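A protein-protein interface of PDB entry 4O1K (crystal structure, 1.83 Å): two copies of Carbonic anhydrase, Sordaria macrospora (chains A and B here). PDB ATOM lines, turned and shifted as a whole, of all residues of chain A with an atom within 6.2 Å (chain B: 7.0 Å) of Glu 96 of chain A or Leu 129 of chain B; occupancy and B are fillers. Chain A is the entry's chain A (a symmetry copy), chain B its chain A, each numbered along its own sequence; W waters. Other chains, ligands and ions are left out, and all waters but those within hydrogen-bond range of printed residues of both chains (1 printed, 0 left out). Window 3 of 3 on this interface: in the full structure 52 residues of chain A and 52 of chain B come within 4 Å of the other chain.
Among the printed residues, pairs that only touch across the chains: Tyr 97 of chain A with Met 130 of chain B (3.6 Å), Glu 96 of chain A with Leu 129 of chain B (3.7 Å), Leu 89 of chain A with Leu 129 of chain B (3.7 Å), Ser 93 of chain A with Trp 133 of chain B (3.8 Å), Leu 89 of chain A with Pro 132 of chain B (3.8 Å), Leu 89 of chain A with Trp 133 of chain B (3.9 Å), His 101 of chain A with Leu 127 of chain B (3.97 Å) and Ser 93 of chain A with Leu 129 of chain B (3.98 Å).
Glu 96 of chain A touches just one residue of chain B: Leu 129 (3.7 Å).
Printed residues of chain A within 4 Å of Leu 129 of chain B: Leu 89, Ser 93 and Glu 96.
Printed residues of chain B within 4 Å of Tyr 97 of chain A: Met 130 (3.6 Å).
Printed residues of chain B within 4 Å of Leu 89 of chain A: Leu 129 (3.7 Å), Pro 132 (3.8 Å) and Trp 133 (3.9 Å).
Of the printed residues of chain A, Met 130 of chain B touches Ser 93 and Tyr 97.
Of the printed residues of chain B, His 101 of chain A touches Leu 127.
Of the printed residues of chain A, Pro 132 of chain B touches Leu 89 (3.8 Å).
The nearest residue of chain B that does not touch Glu 96 of chain A is Leu 127 of chain B (4.2 Å).
The nearest printed residue of chain A that does not touch Leu 129 of chain B is Met 92 of chain A (4.2 Å).
The backbone carbonyl oxygen (O) of Ser 93 of chain A sits close to the side-chain sulfur (SD) of Met 130 of chain B (3.1 Å).
The backbone carbonyl oxygen (O) of Leu 89 of chain A is in hydrogen-bond range of the side-chain hydroxyl (OG) of Ser 93 of chain A, at 2.6 Å.
The backbone NH (N) of Leu 127 of chain B lies within hydrogen-bond range of the side-chain amide oxygen (OD1) of Asn 131 of chain B, 2.7 Å away.
The backbone NH (N) of Leu 102 of chain A sits at hydrogen-bond distance from the backbone carbonyl oxygen (O) of Tyr 97 of chain A, at 3.0 Å.
Of the 9 printed residues of chain B, 5 touch a printed residue of chain A.
Along chain B the printed residues that touch a printed residue of chain A span positions 127 to 133.
Printed residues of chain A that touch a printed residue of chain B: Leu 89, Ser 93, Glu 96, Tyr 97 and His 101.
Hydrophobic or aromatic side chains of chain A that line the printed part of chain B: Leu 89, Tyr 97 and His 101.
No position is printed for both chains.
Water W1 lies within hydrogen-bond range of a ring nitrogen (NE2) of His 101 of chain A (2.4 Å), the backbone carbonyl oxygen (O) of Leu 127 of chain B (2.9 Å) and the side-chain carboxylate (OE2) of Glu 96 of chain A (3.4 Å).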
ATOM      1  N   LEU A  52     -35.516 -23.306  36.319  1.00  0.00           N
ATOM      2  CA  LEU A  52     -35.303 -23.516  34.890  1.00  0.00           C
ATOM      3  C   LEU A  52     -36.134 -24.744  34.488  1.00  0.00           C
ATOM      4  O   LEU A  52     -36.007 -25.807  35.079  1.00  0.00           O
ATOM      5  CB  LEU A  52     -33.825 -23.794  34.584  1.00  0.00           C
ATOM      6  CG  LEU A  52     -33.531 -24.312  33.173  1.00  0.00           C
ATOM      7  CD1 LEU A  52     -33.987 -23.320  32.090  1.00  0.00           C
ATOM      8  CD2 LEU A  52     -32.049 -24.643  32.983  1.00  0.00           C
ATOM      9  N   LEU A  89     -25.796 -25.427  21.612  1.00  0.00           N
ATOM     10  CA  LEU A  89     -25.504 -24.163  22.323  1.00  0.00           C
ATOM     11  C   LEU A  89     -26.758 -23.498  22.841  1.00  0.00           C
ATOM     12  O   LEU A  89     -26.720 -22.751  23.813  1.00  0.00           O
ATOM     13  CB  LEU A  89     -24.844 -23.186  21.369  1.00  0.00           C
ATOM     14  CG  LEU A  89     -24.286 -21.934  22.031  1.00  0.00           C
ATOM     15  CD1 LEU A  89     -23.275 -22.382  23.099  1.00  0.00           C
ATOM     16  CD2 LEU A  89     -23.653 -20.979  20.990  1.00  0.00           C
ATOM     17  N   VAL A  91     -29.558 -24.852  24.297  1.00  0.00           N
ATOM     18  CA  VAL A  91     -29.845 -25.336  25.655  1.00  0.00           C
ATOM     19  C   VAL A  91     -28.665 -25.185  26.602  1.00  0.00           C
ATOM     20  O   VAL A  91     -28.854 -24.881  27.794  1.00  0.00           O
ATOM     21  CB  VAL A  91     -30.386 -26.805  25.675  1.00  0.00           C
ATOM     22  CG1 VAL A  91     -29.260 -27.816  25.525  1.00  0.00           C
ATOM     23  CG2 VAL A  91     -31.109 -27.112  26.973  1.00  0.00           C
ATOM     24  N   MET A  92     -27.452 -25.407  26.100  1.00  0.00           N
ATOM     25  CA  MET A  92     -26.296 -25.307  26.990  1.00  0.00           C
ATOM     26  C   MET A  92     -26.143 -23.894  27.529  1.00  0.00           C
ATOM     27  O   MET A  92     -25.872 -23.673  28.724  1.00  0.00           O
ATOM     28  CB  MET A  92     -25.024 -25.740  26.278  1.00  0.00           C
ATOM     29  CG  MET A  92     -24.979 -27.214  26.007  1.00  0.00           C
ATOM     30  SD  MET A  92     -24.803 -28.073  27.600  1.00  0.00           S
ATOM     31  CE  MET A  92     -26.389 -28.857  27.665  1.00  0.00           C
ATOM     32  N   SER A  93     -26.371 -22.926  26.660  1.00  0.00           N
ATOM     33  CA  SER A  93     -26.240 -21.543  27.074  1.00  0.00           C
ATOM     34  C   SER A  93     -27.405 -21.186  27.990  1.00  0.00           C
ATOM     35  O   SER A  93     -27.240 -20.417  28.959  1.00  0.00           O
ATOM     36  CB  SER A  93     -26.142 -20.608  25.859  1.00  0.00           C
ATOM     37  OG  SER A  93     -27.334 -20.644  25.121  1.00  0.00           O
ATOM     38  N   VAL A  94     -28.583 -21.754  27.747  1.00  0.00           N
ATOM     39  CA  VAL A  94     -29.616 -21.470  28.741  1.00  0.00           C
ATOM     40  C   VAL A  94     -29.403 -22.104  30.155  1.00  0.00           C
ATOM     41  O   VAL A  94     -29.747 -21.485  31.178  1.00  0.00           O
ATOM     42  CB  VAL A  94     -31.006 -21.671  28.196  1.00  0.00           C
ATOM     43  CG1 VAL A  94     -31.365 -23.105  28.140  1.00  0.00           C
ATOM     44  CG2 VAL A  94     -31.945 -20.997  29.092  1.00  0.00           C
ATOM     45  N   ILE A  95     -28.815 -23.297  30.223  1.00  0.00           N
ATOM     46  CA  ILE A  95     -28.480 -23.908  31.516  1.00  0.00           C
ATOM     47  C   ILE A  95     -27.421 -23.054  32.203  1.00  0.00           C
ATOM     48  O   ILE A  95     -27.524 -22.699  33.407  1.00  0.00           O
ATOM     49  CB  ILE A  95     -27.960 -25.345  31.309  1.00  0.00           C
ATOM     50  CG1 ILE A  95     -29.098 -26.208  30.769  1.00  0.00           C
ATOM     51  CG2 ILE A  95     -27.404 -25.939  32.622  1.00  0.00           C
ATOM     52  CD1 ILE A  95     -28.697 -27.649  30.423  1.00  0.00           C
ATOM     53  N   GLU A  96     -26.388 -22.715  31.445  1.00  0.00           N
ATOM     54  CA  GLU A  96     -25.323 -21.874  31.984  1.00  0.00           C
ATOM     55  C   GLU A  96     -25.877 -20.569  32.561  1.00  0.00           C
ATOM     56  O   GLU A  96     -25.535 -20.169  33.687  1.00  0.00           O
ATOM     57  CB  GLU A  96     -24.330 -21.560  30.862  1.00  0.00           C
ATOM     58  CG  GLU A  96     -23.344 -20.449  31.188  1.00  0.00           C
ATOM     59  CD  GLU A  96     -22.050 -20.997  31.728  1.00  0.00           C
ATOM     60  OE1 GLU A  96     -22.129 -21.950  32.524  1.00  0.00           O
ATOM     61  OE2 GLU A  96     -20.971 -20.490  31.345  1.00  0.00           O
ATOM     62  N   TYR A  97     -26.747 -19.919  31.792  1.00  0.00           N
ATOM     63  CA  TYR A  97     -27.321 -18.625  32.163  1.00  0.00           C
ATOM     64  C   TYR A  97     -28.257 -18.704  33.359  1.00  0.00           C
ATOM     65  O   TYR A  97     -28.256 -17.820  34.230  1.00  0.00           O
ATOM     66  CB  TYR A  97     -28.075 -18.044  30.967  1.00  0.00           C
ATOM     67  CG  TYR A  97     -28.663 -16.657  31.173  1.00  0.00           C
ATOM     68  CD1 TYR A  97     -27.850 -15.536  31.335  1.00  0.00           C
ATOM     69  CD2 TYR A  97     -30.031 -16.468  31.154  1.00  0.00           C
ATOM     70  CE1 TYR A  97     -28.411 -14.263  31.496  1.00  0.00           C
ATOM     71  CE2 TYR A  97     -30.594 -15.223  31.310  1.00  0.00           C
ATOM     72  CZ  TYR A  97     -29.793 -14.128  31.477  1.00  0.00           C
ATOM     73  OH  TYR A  97     -30.412 -12.909  31.635  1.00  0.00           O
ATOM     74  N   ALA A  98     -29.054 -19.764  33.404  1.00  0.00           N
ATOM     75  CA  ALA A  98     -29.999 -19.976  34.502  1.00  0.00           C
ATOM     76  C   ALA A  98     -29.276 -20.280  35.801  1.00  0.00           C
ATOM     77  O   ALA A  98     -29.659 -19.789  36.872  1.00  0.00           O
ATOM     78  CB  ALA A  98     -30.976 -21.103  34.159  1.00  0.00           C
ATOM     79  N   VAL A  99     -28.229 -21.094  35.723  1.00  0.00           N
ATOM     80  CA  VAL A  99     -27.530 -21.504  36.943  1.00  0.00           C
ATOM     81  C   VAL A  99     -26.627 -20.398  37.450  1.00  0.00           C
ATOM     82  O   VAL A  99     -26.633 -20.050  38.635  1.00  0.00           O
ATOM     83  CB  VAL A  99     -26.674 -22.717  36.683  1.00  0.00           C
ATOM     84  CG1 VAL A  99     -25.766 -22.966  37.857  1.00  0.00           C
ATOM     85  CG2 VAL A  99     -27.570 -23.936  36.401  1.00  0.00           C
ATOM     86  N   LYS A 100     -25.834 -19.844  36.549  1.00  0.00           N
ATOM     87  CA  LYS A 100     -24.788 -18.918  36.969  1.00  0.00           C
ATOM     88  C   LYS A 100     -25.257 -17.481  37.168  1.00  0.00           C
ATOM     89  O   LYS A 100     -24.815 -16.801  38.096  1.00  0.00           O
ATOM     90  CB  LYS A 100     -23.602 -18.981  36.003  1.00  0.00           C
ATOM     91  CG  LYS A 100     -22.496 -19.899  36.515  1.00  0.00           C
ATOM     92  CD  LYS A 100     -21.547 -20.351  35.413  1.00  0.00           C
ATOM     93  CE  LYS A 100     -20.263 -20.918  36.012  1.00  0.00           C
ATOM     94  NZ  LYS A 100     -19.065 -20.578  35.179  1.00  0.00           N
ATOM     95  N   HIS A 101     -26.159 -17.018  36.314  1.00  0.00           N
ATOM     96  CA  HIS A 101     -26.559 -15.620  36.341  1.00  0.00           C
ATOM     97  C   HIS A 101     -27.951 -15.393  36.937  1.00  0.00           C
ATOM     98  O   HIS A 101     -28.188 -14.373  37.588  1.00  0.00           O
ATOM     99  CB  HIS A 101     -26.424 -15.022  34.940  1.00  0.00           C
ATOM    100  CG  HIS A 101     -25.035 -15.133  34.383  1.00  0.00           C
ATOM    101  ND1 HIS A 101     -23.973 -14.408  34.881  1.00  0.00           N
ATOM    102  CD2 HIS A 101     -24.531 -15.899  33.382  1.00  0.00           C
ATOM    103  CE1 HIS A 101     -22.876 -14.721  34.209  1.00  0.00           C
ATOM    104  NE2 HIS A 101     -23.189 -15.622  33.294  1.00  0.00           N
ATOM    105  N   LEU A 102     -28.870 -16.340  36.751  1.00  0.00           N
ATOM    106  CA  LEU A 102     -30.181 -16.224  37.402  1.00  0.00           C
ATOM    107  C   LEU A 102     -30.228 -16.894  38.781  1.00  0.00           C
ATOM    108  O   LEU A 102     -31.121 -16.598  39.581  1.00  0.00           O
ATOM    109  CB  LEU A 102     -31.309 -16.757  36.498  1.00  0.00           C
ATOM    110  CG  LEU A 102     -31.595 -15.928  35.236  1.00  0.00           C
ATOM    111  CD1 LEU A 102     -32.629 -16.601  34.331  1.00  0.00           C
ATOM    112  CD2 LEU A 102     -32.061 -14.543  35.611  1.00  0.00           C
ATOM    113  N   ALA A 177     -20.652 -28.140  33.787  1.00  0.00           N
ATOM    114  CA  ALA A 177     -19.743 -27.550  34.765  1.00  0.00           C
ATOM    115  C   ALA A 177     -20.481 -26.586  35.685  1.00  0.00           C
ATOM    116  O   ALA A 177     -20.215 -26.545  36.892  1.00  0.00           O
ATOM    117  CB  ALA A 177     -18.565 -26.838  34.053  1.00  0.00           C
ATOM    118  N   ALA A 178     -21.418 -25.834  35.110  1.00  0.00           N
ATOM    119  CA  ALA A 178     -22.177 -24.833  35.857  1.00  0.00           C
ATOM    120  C   ALA A 178     -22.895 -25.510  37.009  1.00  0.00           C
ATOM    121  O   ALA A 178     -22.773 -25.093  38.183  1.00  0.00           O
ATOM    122  CB  ALA A 178     -23.185 -24.155  34.935  1.00  0.00           C
ATOM    123  N   GLN A 181     -20.408 -27.022  39.752  1.00  0.00           N
ATOM    124  CA  GLN A 181     -19.787 -25.957  40.537  1.00  0.00           C
ATOM    125  C   GLN A 181     -20.787 -25.349  41.515  1.00  0.00           C
ATOM    126  O   GLN A 181     -20.517 -25.279  42.726  1.00  0.00           O
ATOM    127  CB  GLN A 181     -19.208 -24.880  39.617  1.00  0.00           C
ATOM    128  CG  GLN A 181     -17.951 -25.326  38.849  1.00  0.00           C
ATOM    129  CD  GLN A 181     -17.678 -24.468  37.627  1.00  0.00           C
ATOM    130  OE1 GLN A 181     -18.588 -23.843  37.074  1.00  0.00           O
ATOM    131  NE2 GLN A 181     -16.425 -24.439  37.192  1.00  0.00           N
ATOM    132  N   ASP B 126     -17.563 -10.869  29.694  1.00  0.00           N
ATOM    133  CA  ASP B 126     -17.327 -12.270  29.392  1.00  0.00           C
ATOM    134  C   ASP B 126     -18.393 -13.115  30.097  1.00  0.00           C
ATOM    135  O   ASP B 126     -18.387 -13.238  31.329  1.00  0.00           O
ATOM    136  CB  ASP B 126     -15.927 -12.663  29.861  1.00  0.00           C
ATOM    137  CG  ASP B 126     -15.465 -13.986  29.284  1.00  0.00           C
ATOM    138  OD1 ASP B 126     -16.283 -14.697  28.662  1.00  0.00           O
ATOM    139  OD2 ASP B 126     -14.274 -14.327  29.476  1.00  0.00           O
ATOM    140  N   LEU B 127     -19.320 -13.668  29.313  1.00  0.00           N
ATOM    141  CA  LEU B 127     -20.412 -14.482  29.858  1.00  0.00           C
ATOM    142  C   LEU B 127     -20.249 -15.960  29.483  1.00  0.00           C
ATOM    143  O   LEU B 127     -21.225 -16.714  29.459  1.00  0.00           O
ATOM    144  CB  LEU B 127     -21.775 -13.957  29.396  1.00  0.00           C
ATOM    145  CG  LEU B 127     -22.534 -13.032  30.351  1.00  0.00           C
ATOM    146  CD1 LEU B 127     -21.569 -12.198  31.146  1.00  0.00           C
ATOM    147  CD2 LEU B 127     -23.509 -12.139  29.639  1.00  0.00           C
ATOM    148  N   GLY B 128     -19.015 -16.362  29.190  1.00  0.00           N
ATOM    149  CA  GLY B 128     -18.708 -17.760  28.902  1.00  0.00           C
ATOM    150  C   GLY B 128     -19.456 -18.312  27.704  1.00  0.00           C
ATOM    151  O   GLY B 128     -19.415 -17.724  26.618  1.00  0.00           O
ATOM    152  N   LEU B 129     -20.137 -19.439  27.922  1.00  0.00           N
ATOM    153  CA  LEU B 129     -20.981 -20.105  26.926  1.00  0.00           C
ATOM    154  C   LEU B 129     -22.015 -19.202  26.304  1.00  0.00           C
ATOM    155  O   LEU B 129     -22.413 -19.403  25.152  1.00  0.00           O
ATOM    156  CB  LEU B 129     -21.710 -21.293  27.568  1.00  0.00           C
ATOM    157  CG  LEU B 129     -20.982 -22.628  27.568  1.00  0.00           C
ATOM    158  CD1 LEU B 129     -21.732 -23.687  28.363  1.00  0.00           C
ATOM    159  CD2 LEU B 129     -20.850 -23.062  26.147  1.00  0.00           C
ATOM    160  N   MET B 130     -22.501 -18.230  27.070  1.00  0.00           N
ATOM    161  CA  MET B 130     -23.495 -17.321  26.536  1.00  0.00           C
ATOM    162  C   MET B 130     -22.925 -16.424  25.431  1.00  0.00           C
ATOM    163  O   MET B 130     -23.695 -15.906  24.611  1.00  0.00           O
ATOM    164  CB  MET B 130     -24.104 -16.458  27.645  1.00  0.00           C
ATOM    165  CG  MET B 130     -25.122 -17.191  28.533  1.00  0.00           C
ATOM    166  SD  MET B 130     -26.635 -17.640  27.640  1.00  0.00           S
ATOM    167  CE  MET B 130     -27.106 -16.081  26.916  1.00  0.00           C
ATOM    168  N   ASN B 131     -21.599 -16.238  25.390  1.00  0.00           N
ATOM    169  CA  ASN B 131     -21.053 -15.241  24.479  1.00  0.00           C
ATOM    170  C   ASN B 131     -21.445 -15.499  23.019  1.00  0.00           C
ATOM    171  O   ASN B 131     -21.956 -14.605  22.372  1.00  0.00           O
ATOM    172  CB  ASN B 131     -19.522 -15.087  24.609  1.00  0.00           C
ATOM    173  CG  ASN B 131     -19.075 -14.612  25.994  1.00  0.00           C
ATOM    174  OD1 ASN B 131     -19.783 -13.881  26.687  1.00  0.00           O
ATOM    175  ND2 ASN B 131     -17.867 -15.009  26.384  1.00  0.00           N
ATOM    176  N   PRO B 132     -21.204 -16.713  22.497  1.00  0.00           N
ATOM    177  CA  PRO B 132     -21.546 -16.821  21.075  1.00  0.00           C
ATOM    178  C   PRO B 132     -23.067 -16.782  20.852  1.00  0.00           C
ATOM    179  O   PRO B 132     -23.514 -16.396  19.762  1.00  0.00           O
ATOM    180  CB  PRO B 132     -21.018 -18.203  20.690  1.00  0.00           C
ATOM    181  CG  PRO B 132     -20.258 -18.717  21.865  1.00  0.00           C
ATOM    182  CD  PRO B 132     -20.767 -18.002  23.050  1.00  0.00           C
ATOM    183  N   TRP B 133     -23.860 -17.150  21.859  1.00  0.00           N
ATOM    184  CA  TRP B 133     -25.312 -17.015  21.683  1.00  0.00           C
ATOM    185  C   TRP B 133     -25.736 -15.552  21.584  1.00  0.00           C
ATOM    186  O   TRP B 133     -26.423 -15.152  20.630  1.00  0.00           O
ATOM    187  CB  TRP B 133     -26.062 -17.759  22.803  1.00  0.00           C
ATOM    188  CG  TRP B 133     -27.521 -17.846  22.532  1.00  0.00           C
ATOM    189  CD1 TRP B 133     -28.498 -17.054  23.046  1.00  0.00           C
ATOM    190  CD2 TRP B 133     -28.174 -18.798  21.683  1.00  0.00           C
ATOM    191  NE1 TRP B 133     -29.727 -17.439  22.557  1.00  0.00           N
ATOM    192  CE2 TRP B 133     -29.550 -18.522  21.718  1.00  0.00           C
ATOM    193  CE3 TRP B 133     -27.719 -19.860  20.891  1.00  0.00           C
ATOM    194  CZ2 TRP B 133     -30.479 -19.269  21.001  1.00  0.00           C
ATOM    195  CZ3 TRP B 133     -28.647 -20.604  20.163  1.00  0.00           C
ATOM    196  CH2 TRP B 133     -30.010 -20.290  20.213  1.00  0.00           C
ATOM    197  N   LEU B 134     -25.332 -14.737  22.556  1.00  0.00           N
ATOM    198  CA  LEU B 134     -25.670 -13.319  22.548  1.00  0.00           C
ATOM    199  C   LEU B 134     -25.026 -12.553  21.411  1.00  0.00           C
ATOM    200  O   LEU B 134     -25.500 -11.474  21.026  1.00  0.00           O
ATOM    201  CB  LEU B 134     -25.263 -12.692  23.861  1.00  0.00           C
ATOM    202  CG  LEU B 134     -25.961 -13.343  25.034  1.00  0.00           C
ATOM    203  CD1 LEU B 134     -25.418 -12.798  26.336  1.00  0.00           C
ATOM    204  CD2 LEU B 134     -27.450 -13.119  24.928  1.00  0.00           C
HETATM  205  O   HOH W   1     -21.854 -17.340  32.181  1.00  0.00           O
